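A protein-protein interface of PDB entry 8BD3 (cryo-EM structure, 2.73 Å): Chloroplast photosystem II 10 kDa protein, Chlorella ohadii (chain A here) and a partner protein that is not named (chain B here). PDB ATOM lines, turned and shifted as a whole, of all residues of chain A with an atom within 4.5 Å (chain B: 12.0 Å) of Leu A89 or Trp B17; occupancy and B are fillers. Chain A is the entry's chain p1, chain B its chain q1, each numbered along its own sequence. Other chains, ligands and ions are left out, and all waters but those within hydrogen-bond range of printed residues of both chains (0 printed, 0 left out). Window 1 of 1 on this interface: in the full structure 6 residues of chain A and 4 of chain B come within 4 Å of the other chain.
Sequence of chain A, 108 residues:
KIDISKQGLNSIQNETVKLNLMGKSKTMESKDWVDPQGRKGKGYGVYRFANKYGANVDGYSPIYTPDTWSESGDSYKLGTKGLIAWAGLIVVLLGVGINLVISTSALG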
ATOM      1  N   GLY A  82      -3.738   7.752 -21.848  1.00  0.00           N
ATOM      2  CA  GLY A  82      -2.498   7.428 -22.529  1.00  0.00           C
ATOM      3  C   GLY A  82      -2.326   5.937 -22.740  1.00  0.00           C
ATOM      4  O   GLY A  82      -1.606   5.507 -23.642  1.00  0.00           O
ATOM      5  N   ALA A  85      -4.443   4.961 -25.827  1.00  0.00           N
ATOM      6  CA  ALA A  85      -3.709   5.478 -26.976  1.00  0.00           C
ATOM      7  C   ALA A  85      -2.491   4.616 -27.275  1.00  0.00           C
ATOM      8  O   ALA A  85      -2.138   4.411 -28.442  1.00  0.00           O
ATOM      9  CB  ALA A  85      -3.294   6.927 -26.730  1.00  0.00           C
ATOM     10  N   TRP A  86      -1.831   4.112 -26.232  1.00  0.00           N
ATOM     11  CA  TRP A  86      -0.724   3.183 -26.429  1.00  0.00           C
ATOM     12  C   TRP A  86      -1.198   1.900 -27.095  1.00  0.00           C
ATOM     13  O   TRP A  86      -0.555   1.394 -28.021  1.00  0.00           O
ATOM     14  CB  TRP A  86      -0.059   2.877 -25.089  1.00  0.00           C
ATOM     15  CG  TRP A  86       0.853   1.701 -25.137  1.00  0.00           C
ATOM     16  CD1 TRP A  86       2.144   1.686 -25.562  1.00  0.00           C
ATOM     17  CD2 TRP A  86       0.546   0.362 -24.738  1.00  0.00           C
ATOM     18  NE1 TRP A  86       2.663   0.422 -25.459  1.00  0.00           N
ATOM     19  CE2 TRP A  86       1.700  -0.411 -24.955  1.00  0.00           C
ATOM     20  CE3 TRP A  86      -0.594  -0.258 -24.225  1.00  0.00           C
ATOM     21  CZ2 TRP A  86       1.747  -1.773 -24.676  1.00  0.00           C
ATOM     22  CZ3 TRP A  86      -0.546  -1.609 -23.948  1.00  0.00           C
ATOM     23  CH2 TRP A  86       0.617  -2.352 -24.173  1.00  0.00           C
ATOM     24  N   ALA A  87      -2.326   1.355 -26.634  1.00  0.00           N
ATOM     25  CA  ALA A  87      -2.843   0.124 -27.219  1.00  0.00           C
ATOM     26  C   ALA A  87      -3.251   0.338 -28.668  1.00  0.00           C
ATOM     27  O   ALA A  87      -3.009  -0.518 -29.527  1.00  0.00           O
ATOM     28  CB  ALA A  87      -4.022  -0.396 -26.396  1.00  0.00           C
ATOM     29  N   GLY A  88      -3.879   1.476 -28.960  1.00  0.00           N
ATOM     30  CA  GLY A  88      -4.251   1.764 -30.336  1.00  0.00           C
ATOM     31  C   GLY A  88      -3.045   1.896 -31.244  1.00  0.00           C
ATOM     32  O   GLY A  88      -3.025   1.365 -32.355  1.00  0.00           O
ATOM     33  N   LEU A  89      -2.014   2.604 -30.776  1.00  0.00           N
ATOM     34  CA  LEU A  89      -0.825   2.808 -31.595  1.00  0.00           C
ATOM     35  C   LEU A  89      -0.071   1.502 -31.813  1.00  0.00           C
ATOM     36  O   LEU A  89       0.497   1.278 -32.888  1.00  0.00           O
ATOM     37  CB  LEU A  89       0.080   3.854 -30.946  1.00  0.00           C
ATOM     38  CG  LEU A  89       1.331   4.258 -31.722  1.00  0.00           C
ATOM     39  CD1 LEU A  89       0.970   4.649 -33.138  1.00  0.00           C
ATOM     40  CD2 LEU A  89       2.030   5.404 -31.025  1.00  0.00           C
ATOM     41  N   ILE A  90      -0.056   0.628 -30.805  1.00  0.00           N
ATOM     42  CA  ILE A  90       0.637  -0.653 -30.930  1.00  0.00           C
ATOM     43  C   ILE A  90       0.027  -1.475 -32.057  1.00  0.00           C
ATOM     44  O   ILE A  90       0.738  -2.063 -32.880  1.00  0.00           O
ATOM     45  CB  ILE A  90       0.603  -1.413 -29.594  1.00  0.00           C
ATOM     46  CG1 ILE A  90       1.686  -0.889 -28.657  1.00  0.00           C
ATOM     47  CG2 ILE A  90       0.787  -2.901 -29.814  1.00  0.00           C
ATOM     48  CD1 ILE A  90       3.086  -1.189 -29.131  1.00  0.00           C
ATOM     49  N   VAL A  91      -1.305  -1.522 -32.112  1.00  0.00           N
ATOM     50  CA  VAL A  91      -1.984  -2.278 -33.161  1.00  0.00           C
ATOM     51  C   VAL A  91      -1.694  -1.674 -34.529  1.00  0.00           C
ATOM     52  O   VAL A  91      -1.410  -2.391 -35.496  1.00  0.00           O
ATOM     53  CB  VAL A  91      -3.496  -2.339 -32.881  1.00  0.00           C
ATOM     54  CG1 VAL A  91      -4.222  -3.010 -34.029  1.00  0.00           C
ATOM     55  CG2 VAL A  91      -3.758  -3.075 -31.583  1.00  0.00           C
ATOM     56  N   VAL A  92      -1.761  -0.346 -34.632  1.00  0.00           N
ATOM     57  CA  VAL A  92      -1.557   0.320 -35.918  1.00  0.00           C
ATOM     58  C   VAL A  92      -0.145   0.065 -36.432  1.00  0.00           C
ATOM     59  O   VAL A  92       0.059  -0.276 -37.602  1.00  0.00           O
ATOM     60  CB  VAL A  92      -1.847   1.826 -35.798  1.00  0.00           C
ATOM     61  CG1 VAL A  92      -1.432   2.552 -37.063  1.00  0.00           C
ATOM     62  CG2 VAL A  92      -3.317   2.059 -35.507  1.00  0.00           C
ATOM     63  N   LEU A  93       0.849   0.222 -35.560  1.00  0.00           N
ATOM     64  CA  LEU A  93       2.231   0.028 -35.982  1.00  0.00           C
ATOM     65  C   LEU A  93       2.530  -1.442 -36.237  1.00  0.00           C
ATOM     66  O   LEU A  93       3.379  -1.775 -37.072  1.00  0.00           O
ATOM     67  CB  LEU A  93       3.184   0.600 -34.936  1.00  0.00           C
ATOM     68  CG  LEU A  93       3.122   2.118 -34.790  1.00  0.00           C
ATOM     69  CD1 LEU A  93       4.143   2.606 -33.782  1.00  0.00           C
ATOM     70  CD2 LEU A  93       3.332   2.784 -36.138  1.00  0.00           C
ATOM     71  N   ALA B   8      13.302   5.737 -42.567  1.00  0.00           N
ATOM     72  CA  ALA B   8      13.396   6.896 -41.687  1.00  0.00           C
ATOM     73  C   ALA B   8      12.017   7.391 -41.271  1.00  0.00           C
ATOM     74  O   ALA B   8      11.864   7.988 -40.200  1.00  0.00           O
ATOM     75  CB  ALA B   8      14.186   8.010 -42.371  1.00  0.00           C
ATOM     76  N   LEU B   9      11.006   7.114 -42.095  1.00  0.00           N
ATOM     77  CA  LEU B   9       9.623   7.547 -41.767  1.00  0.00           C
ATOM     78  C   LEU B   9       9.123   6.786 -40.533  1.00  0.00           C
ATOM     79  O   LEU B   9       8.159   7.262 -39.908  1.00  0.00           O
ATOM     80  CB  LEU B   9       8.716   7.297 -42.973  1.00  0.00           C
ATOM     81  CG  LEU B   9       8.074   8.550 -43.567  1.00  0.00           C
ATOM     82  CD1 LEU B   9       7.087   9.163 -42.588  1.00  0.00           C
ATOM     83  CD2 LEU B   9       9.138   9.566 -43.955  1.00  0.00           C
ATOM     84  N   LEU B  10       9.750   5.654 -40.198  1.00  0.00           N
ATOM     85  CA  LEU B  10       9.350   4.923 -39.001  1.00  0.00           C
ATOM     86  C   LEU B  10       9.691   5.696 -37.736  1.00  0.00           C
ATOM     87  O   LEU B  10       9.122   5.425 -36.672  1.00  0.00           O
ATOM     88  CB  LEU B  10      10.025   3.552 -38.970  1.00  0.00           C
ATOM     89  CG  LEU B  10       9.286   2.355 -39.569  1.00  0.00           C
ATOM     90  CD1 LEU B  10       8.897   2.613 -41.011  1.00  0.00           C
ATOM     91  CD2 LEU B  10      10.154   1.119 -39.465  1.00  0.00           C
ATOM     92  N   ALA B  11      10.617   6.649 -37.825  1.00  0.00           N
ATOM     93  CA  ALA B  11      11.026   7.388 -36.638  1.00  0.00           C
ATOM     94  C   ALA B  11       9.956   8.380 -36.200  1.00  0.00           C
ATOM     95  O   ALA B  11       9.798   8.636 -35.002  1.00  0.00           O
ATOM     96  CB  ALA B  11      12.349   8.107 -36.896  1.00  0.00           C
ATOM     97  N   VAL B  12       9.219   8.948 -37.149  1.00  0.00           N
ATOM     98  CA  VAL B  12       8.268  10.020 -36.859  1.00  0.00           C
ATOM     99  C   VAL B  12       7.202   9.564 -35.864  1.00  0.00           C
ATOM    100  O   VAL B  12       6.964  10.273 -34.877  1.00  0.00           O
ATOM    101  CB  VAL B  12       7.631  10.562 -38.150  1.00  0.00           C
ATOM    102  CG1 VAL B  12       6.657  11.677 -37.829  1.00  0.00           C
ATOM    103  CG2 VAL B  12       8.709  11.052 -39.101  1.00  0.00           C
ATOM    104  N   PRO B  13       6.531   8.419 -36.054  1.00  0.00           N
ATOM    105  CA  PRO B  13       5.617   7.961 -34.995  1.00  0.00           C
ATOM    106  C   PRO B  13       6.324   7.652 -33.689  1.00  0.00           C
ATOM    107  O   PRO B  13       5.747   7.845 -32.613  1.00  0.00           O
ATOM    108  CB  PRO B  13       4.975   6.708 -35.606  1.00  0.00           C
ATOM    109  CG  PRO B  13       5.951   6.239 -36.603  1.00  0.00           C
ATOM    110  CD  PRO B  13       6.537   7.481 -37.190  1.00  0.00           C
ATOM    111  N   VAL B  14       7.564   7.168 -33.756  1.00  0.00           N
ATOM    112  CA  VAL B  14       8.299   6.824 -32.542  1.00  0.00           C
ATOM    113  C   VAL B  14       8.707   8.085 -31.792  1.00  0.00           C
ATOM    114  O   VAL B  14       8.502   8.205 -30.580  1.00  0.00           O
ATOM    115  CB  VAL B  14       9.519   5.954 -32.887  1.00  0.00           C
ATOM    116  CG1 VAL B  14      10.409   5.784 -31.676  1.00  0.00           C
ATOM    117  CG2 VAL B  14       9.058   4.611 -33.399  1.00  0.00           C
ATOM    118  N   ILE B  15       9.287   9.050 -32.509  1.00  0.00           N
ATOM    119  CA  ILE B  15       9.709  10.299 -31.879  1.00  0.00           C
ATOM    120  C   ILE B  15       8.503  11.038 -31.317  1.00  0.00           C
ATOM    121  O   ILE B  15       8.548  11.585 -30.209  1.00  0.00           O
ATOM    122  CB  ILE B  15      10.491  11.166 -32.880  1.00  0.00           C
ATOM    123  CG1 ILE B  15      11.791  10.468 -33.282  1.00  0.00           C
ATOM    124  CG2 ILE B  15      10.789  12.532 -32.291  1.00  0.00           C
ATOM    125  CD1 ILE B  15      12.698  10.151 -32.113  1.00  0.00           C
ATOM    126  N   GLY B  16       7.408  11.066 -32.073  1.00  0.00           N
ATOM    127  CA  GLY B  16       6.199  11.704 -31.577  1.00  0.00           C
ATOM    128  C   GLY B  16       5.643  11.015 -30.348  1.00  0.00           C
ATOM    129  O   GLY B  16       5.177  11.667 -29.411  1.00  0.00           O
ATOM    130  N   TRP B  17       5.710   9.681 -30.333  1.00  0.00           N
ATOM    131  CA  TRP B  17       5.162   8.912 -29.184  1.00  0.00           C
ATOM    132  C   TRP B  17       6.027   9.142 -27.941  1.00  0.00           C
ATOM    133  O   TRP B  17       5.454   9.398 -26.866  1.00  0.00           O
ATOM    134  CB  TRP B  17       5.057   7.420 -29.518  1.00  0.00           C
ATOM    135  CG  TRP B  17       4.597   6.590 -28.360  1.00  0.00           C
ATOM    136  CD1 TRP B  17       5.329   5.679 -27.654  1.00  0.00           C
ATOM    137  CD2 TRP B  17       3.293   6.611 -27.752  1.00  0.00           C
ATOM    138  NE1 TRP B  17       4.568   5.124 -26.661  1.00  0.00           N
ATOM    139  CE2 TRP B  17       3.315   5.676 -26.696  1.00  0.00           C
ATOM    140  CE3 TRP B  17       2.113   7.321 -27.999  1.00  0.00           C
ATOM    141  CZ2 TRP B  17       2.202   5.437 -25.892  1.00  0.00           C
ATOM    142  CZ3 TRP B  17       1.015   7.084 -27.205  1.00  0.00           C
ATOM    143  CH2 TRP B  17       1.061   6.156 -26.164  1.00  0.00           C
ATOM    144  N   VAL B  18       7.350   9.046 -28.089  1.00  0.00           N
ATOM    145  CA  VAL B  18       8.265   9.203 -26.920  1.00  0.00           C
ATOM    146  C   VAL B  18       7.991  10.564 -26.280  1.00  0.00           C
ATOM    147  O   VAL B  18       7.834  10.615 -25.048  1.00  0.00           O
ATOM    148  CB  VAL B  18       9.741   9.066 -27.335  1.00  0.00           C
ATOM    149  CG1 VAL B  18      10.682   9.341 -26.173  1.00  0.00           C
ATOM    150  CG2 VAL B  18      10.024   7.703 -27.944  1.00  0.00           C
ATOM    151  N   LEU B  19       7.911  11.615 -27.099  1.00  0.00           N
ATOM    152  CA  LEU B  19       7.639  12.979 -26.577  1.00  0.00           C
ATOM    153  C   LEU B  19       6.297  12.977 -25.843  1.00  0.00           C
ATOM    154  O   LEU B  19       6.249  13.468 -24.701  1.00  0.00           O
ATOM    155  CB  LEU B  19       7.625  13.968 -27.746  1.00  0.00           C
ATOM    156  CG  LEU B  19       8.977  14.578 -28.110  1.00  0.00           C
ATOM    157  CD1 LEU B  19      10.045  13.505 -28.258  1.00  0.00           C
ATOM    158  CD2 LEU B  19       8.873  15.407 -29.380  1.00  0.00           C
ATOM    159  N   PHE B  20       5.252  12.431 -26.472  1.00  0.00           N
ATOM    160  CA  PHE B  20       3.934  12.441 -25.852  1.00  0.00           C
ATOM    161  C   PHE B  20       3.959  11.899 -24.431  1.00  0.00           C
ATOM    162  O   PHE B  20       3.088  12.255 -23.631  1.00  0.00           O
ATOM    163  CB  PHE B  20       2.957  11.637 -26.708  1.00  0.00           C
ATOM    164  CG  PHE B  20       1.582  11.534 -26.125  1.00  0.00           C
ATOM    165  CD1 PHE B  20       0.818  12.665 -25.920  1.00  0.00           C
ATOM    166  CD2 PHE B  20       1.050  10.305 -25.788  1.00  0.00           C
ATOM    167  CE1 PHE B  20      -0.450  12.572 -25.383  1.00  0.00           C
ATOM    168  CE2 PHE B  20      -0.217  10.204 -25.253  1.00  0.00           C
ATOM    169  CZ  PHE B  20      -0.967  11.339 -25.049  1.00  0.00           C
ATOM    170  N   ASN B  21       4.977  11.097 -24.101  1.00  0.00           N
ATOM    171  CA  ASN B  21       5.037  10.461 -22.756  1.00  0.00           C
ATOM    172  C   ASN B  21       6.270  10.929 -21.973  1.00  0.00           C
ATOM    173  O   ASN B  21       6.427  10.467 -20.829  1.00  0.00           O
ATOM    174  CB  ASN B  21       5.064   8.935 -22.852  1.00  0.00           C
ATOM    175  CG  ASN B  21       3.954   8.364 -23.708  1.00  0.00           C
ATOM    176  OD1 ASN B  21       2.994   9.056 -24.035  1.00  0.00           O
ATOM    177  ND2 ASN B  21       4.075   7.098 -24.070  1.00  0.00           N
ATOM    178  N   ILE B  22       7.113  11.793 -22.546  1.00  0.00           N
ATOM    179  CA  ILE B  22       8.379  12.161 -21.837  1.00  0.00           C
ATOM    180  C   ILE B  22       8.559  13.682 -21.796  1.00  0.00           C
ATOM    181  O   ILE B  22       9.238  14.159 -20.869  1.00  0.00           O
ATOM    182  CB  ILE B  22       9.590  11.469 -22.495  1.00  0.00           C
ATOM    183  CG1 ILE B  22      10.693  11.174 -21.476  1.00  0.00           C
ATOM    184  CG2 ILE B  22      10.108  12.281 -23.674  1.00  0.00           C
ATOM    185  CD1 ILE B  22      10.264  10.237 -20.372  1.00  0.00           C
ATOM    186  N   LEU B  23       7.985  14.412 -22.756  1.00  0.00           N
ATOM    187  CA  LEU B  23       8.202  15.883 -22.830  1.00  0.00           C
ATOM    188  C   LEU B  23       7.993  16.523 -21.455  1.00  0.00           C
ATOM    189  O   LEU B  23       8.944  17.151 -20.953  1.00  0.00           O
ATOM    190  CB  LEU B  23       7.227  16.475 -23.851  1.00  0.00           C
ATOM    191  CG  LEU B  23       7.290  17.995 -24.003  1.00  0.00           C
ATOM    192  CD1 LEU B  23       8.709  18.448 -24.310  1.00  0.00           C
ATOM    193  CD2 LEU B  23       6.331  18.472 -25.083  1.00  0.00           C
ATOM    194  N   GLY B  24       6.799  16.381 -20.877  1.00  0.00           N
ATOM    195  CA  GLY B  24       6.501  17.015 -19.616  1.00  0.00           C
ATOM    196  C   GLY B  24       7.552  16.769 -18.552  1.00  0.00           C
ATOM    197  O   GLY B  24       8.110  17.706 -17.976  1.00  0.00           O
ATOM    198  N   PRO B  25       7.834  15.497 -18.254  1.00  0.00           N
ATOM    199  CA  PRO B  25       8.914  15.198 -17.301  1.00  0.00           C
ATOM    200  C   PRO B  25      10.273  15.725 -17.731  1.00  0.00           C
ATOM    201  O   PRO B  25      11.098  16.062 -16.875  1.00  0.00           O
ATOM    202  CB  PRO B  25       8.888  13.668 -17.228  1.00  0.00           C
ATOM    203  CG  PRO B  25       7.495  13.306 -17.560  1.00  0.00           C
ATOM    204  CD  PRO B  25       7.049  14.297 -18.588  1.00  0.00           C
ATOM    205  N   LEU B  26      10.536  15.794 -19.037  1.00  0.00           N
ATOM    206  CA  LEU B  26      11.777  16.396 -19.510  1.00  0.00           C
ATOM    207  C   LEU B  26      11.838  17.876 -19.156  1.00  0.00           C
ATOM    208  O   LEU B  26      12.883  18.383 -18.735  1.00  0.00           O
ATOM    209  CB  LEU B  26      11.919  16.201 -21.018  1.00  0.00           C
ATOM    210  CG  LEU B  26      13.022  17.028 -21.678  1.00  0.00           C
ATOM    211  CD1 LEU B  26      14.378  16.669 -21.099  1.00  0.00           C
ATOM    212  CD2 LEU B  26      13.013  16.850 -23.186  1.00  0.00           C
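The side-chain amide nitrogen of Asn B21 lies close to the indole nitrogen of Trp B17 (3.3 Å).
CH2 of Trp B17 touches O of Gly A82, at 3.7 Å. Trp A86 touches Trp B17. Leu A89 touches Trp B17 (CD2 to CE3, 3.6 Å).
Leu A89 touches just one residue of chain B: Trp B17. Gly A82 touches just one residue of chain B: Trp B17 (3.7 Å). No residue of chain B comes within 4 Å of Ala A85. No residue of chain B comes within 4 Å of Ala A87. No residue of chain B comes within 4 Å of Gly A88. No residue of chain B comes within 4 Å of Ile A90. Printed residues of chain B within 4 Å of Trp A86: Trp B17. Gly B16 touches none of the printed residues of chain A. Ile B15 touches none of the printed residues of chain A. The nearest residue of chain A that does not touch Trp B17 is Ala A85 (4.03 Å). The nearest printed residue of chain B that does not touch Trp A86 is Asn B21 (5.9 Å).
Printed residues of chain B that touch a printed residue of chain A: Trp B17. Hydrophobic or aromatic side chains of chain B within 4 Å of the printed part of chain A: Trp B17. Of the 10 printed residues of chain A, 3 touch a printed residue of chain B. Printed residues of chain A that touch a printed residue of chain B: Gly A82, Trp A86 and Leu A89. Hydrophobic or aromatic side chains of chain A that line the printed part of chain B: Trp A86 and Leu A89. Among the printed residues, 3 pairs touch across the chains. Among the printed residues, no Asp or Glu carboxylate lies within 4 Å of a Lys or Arg side-chain nitrogen of the other chain.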
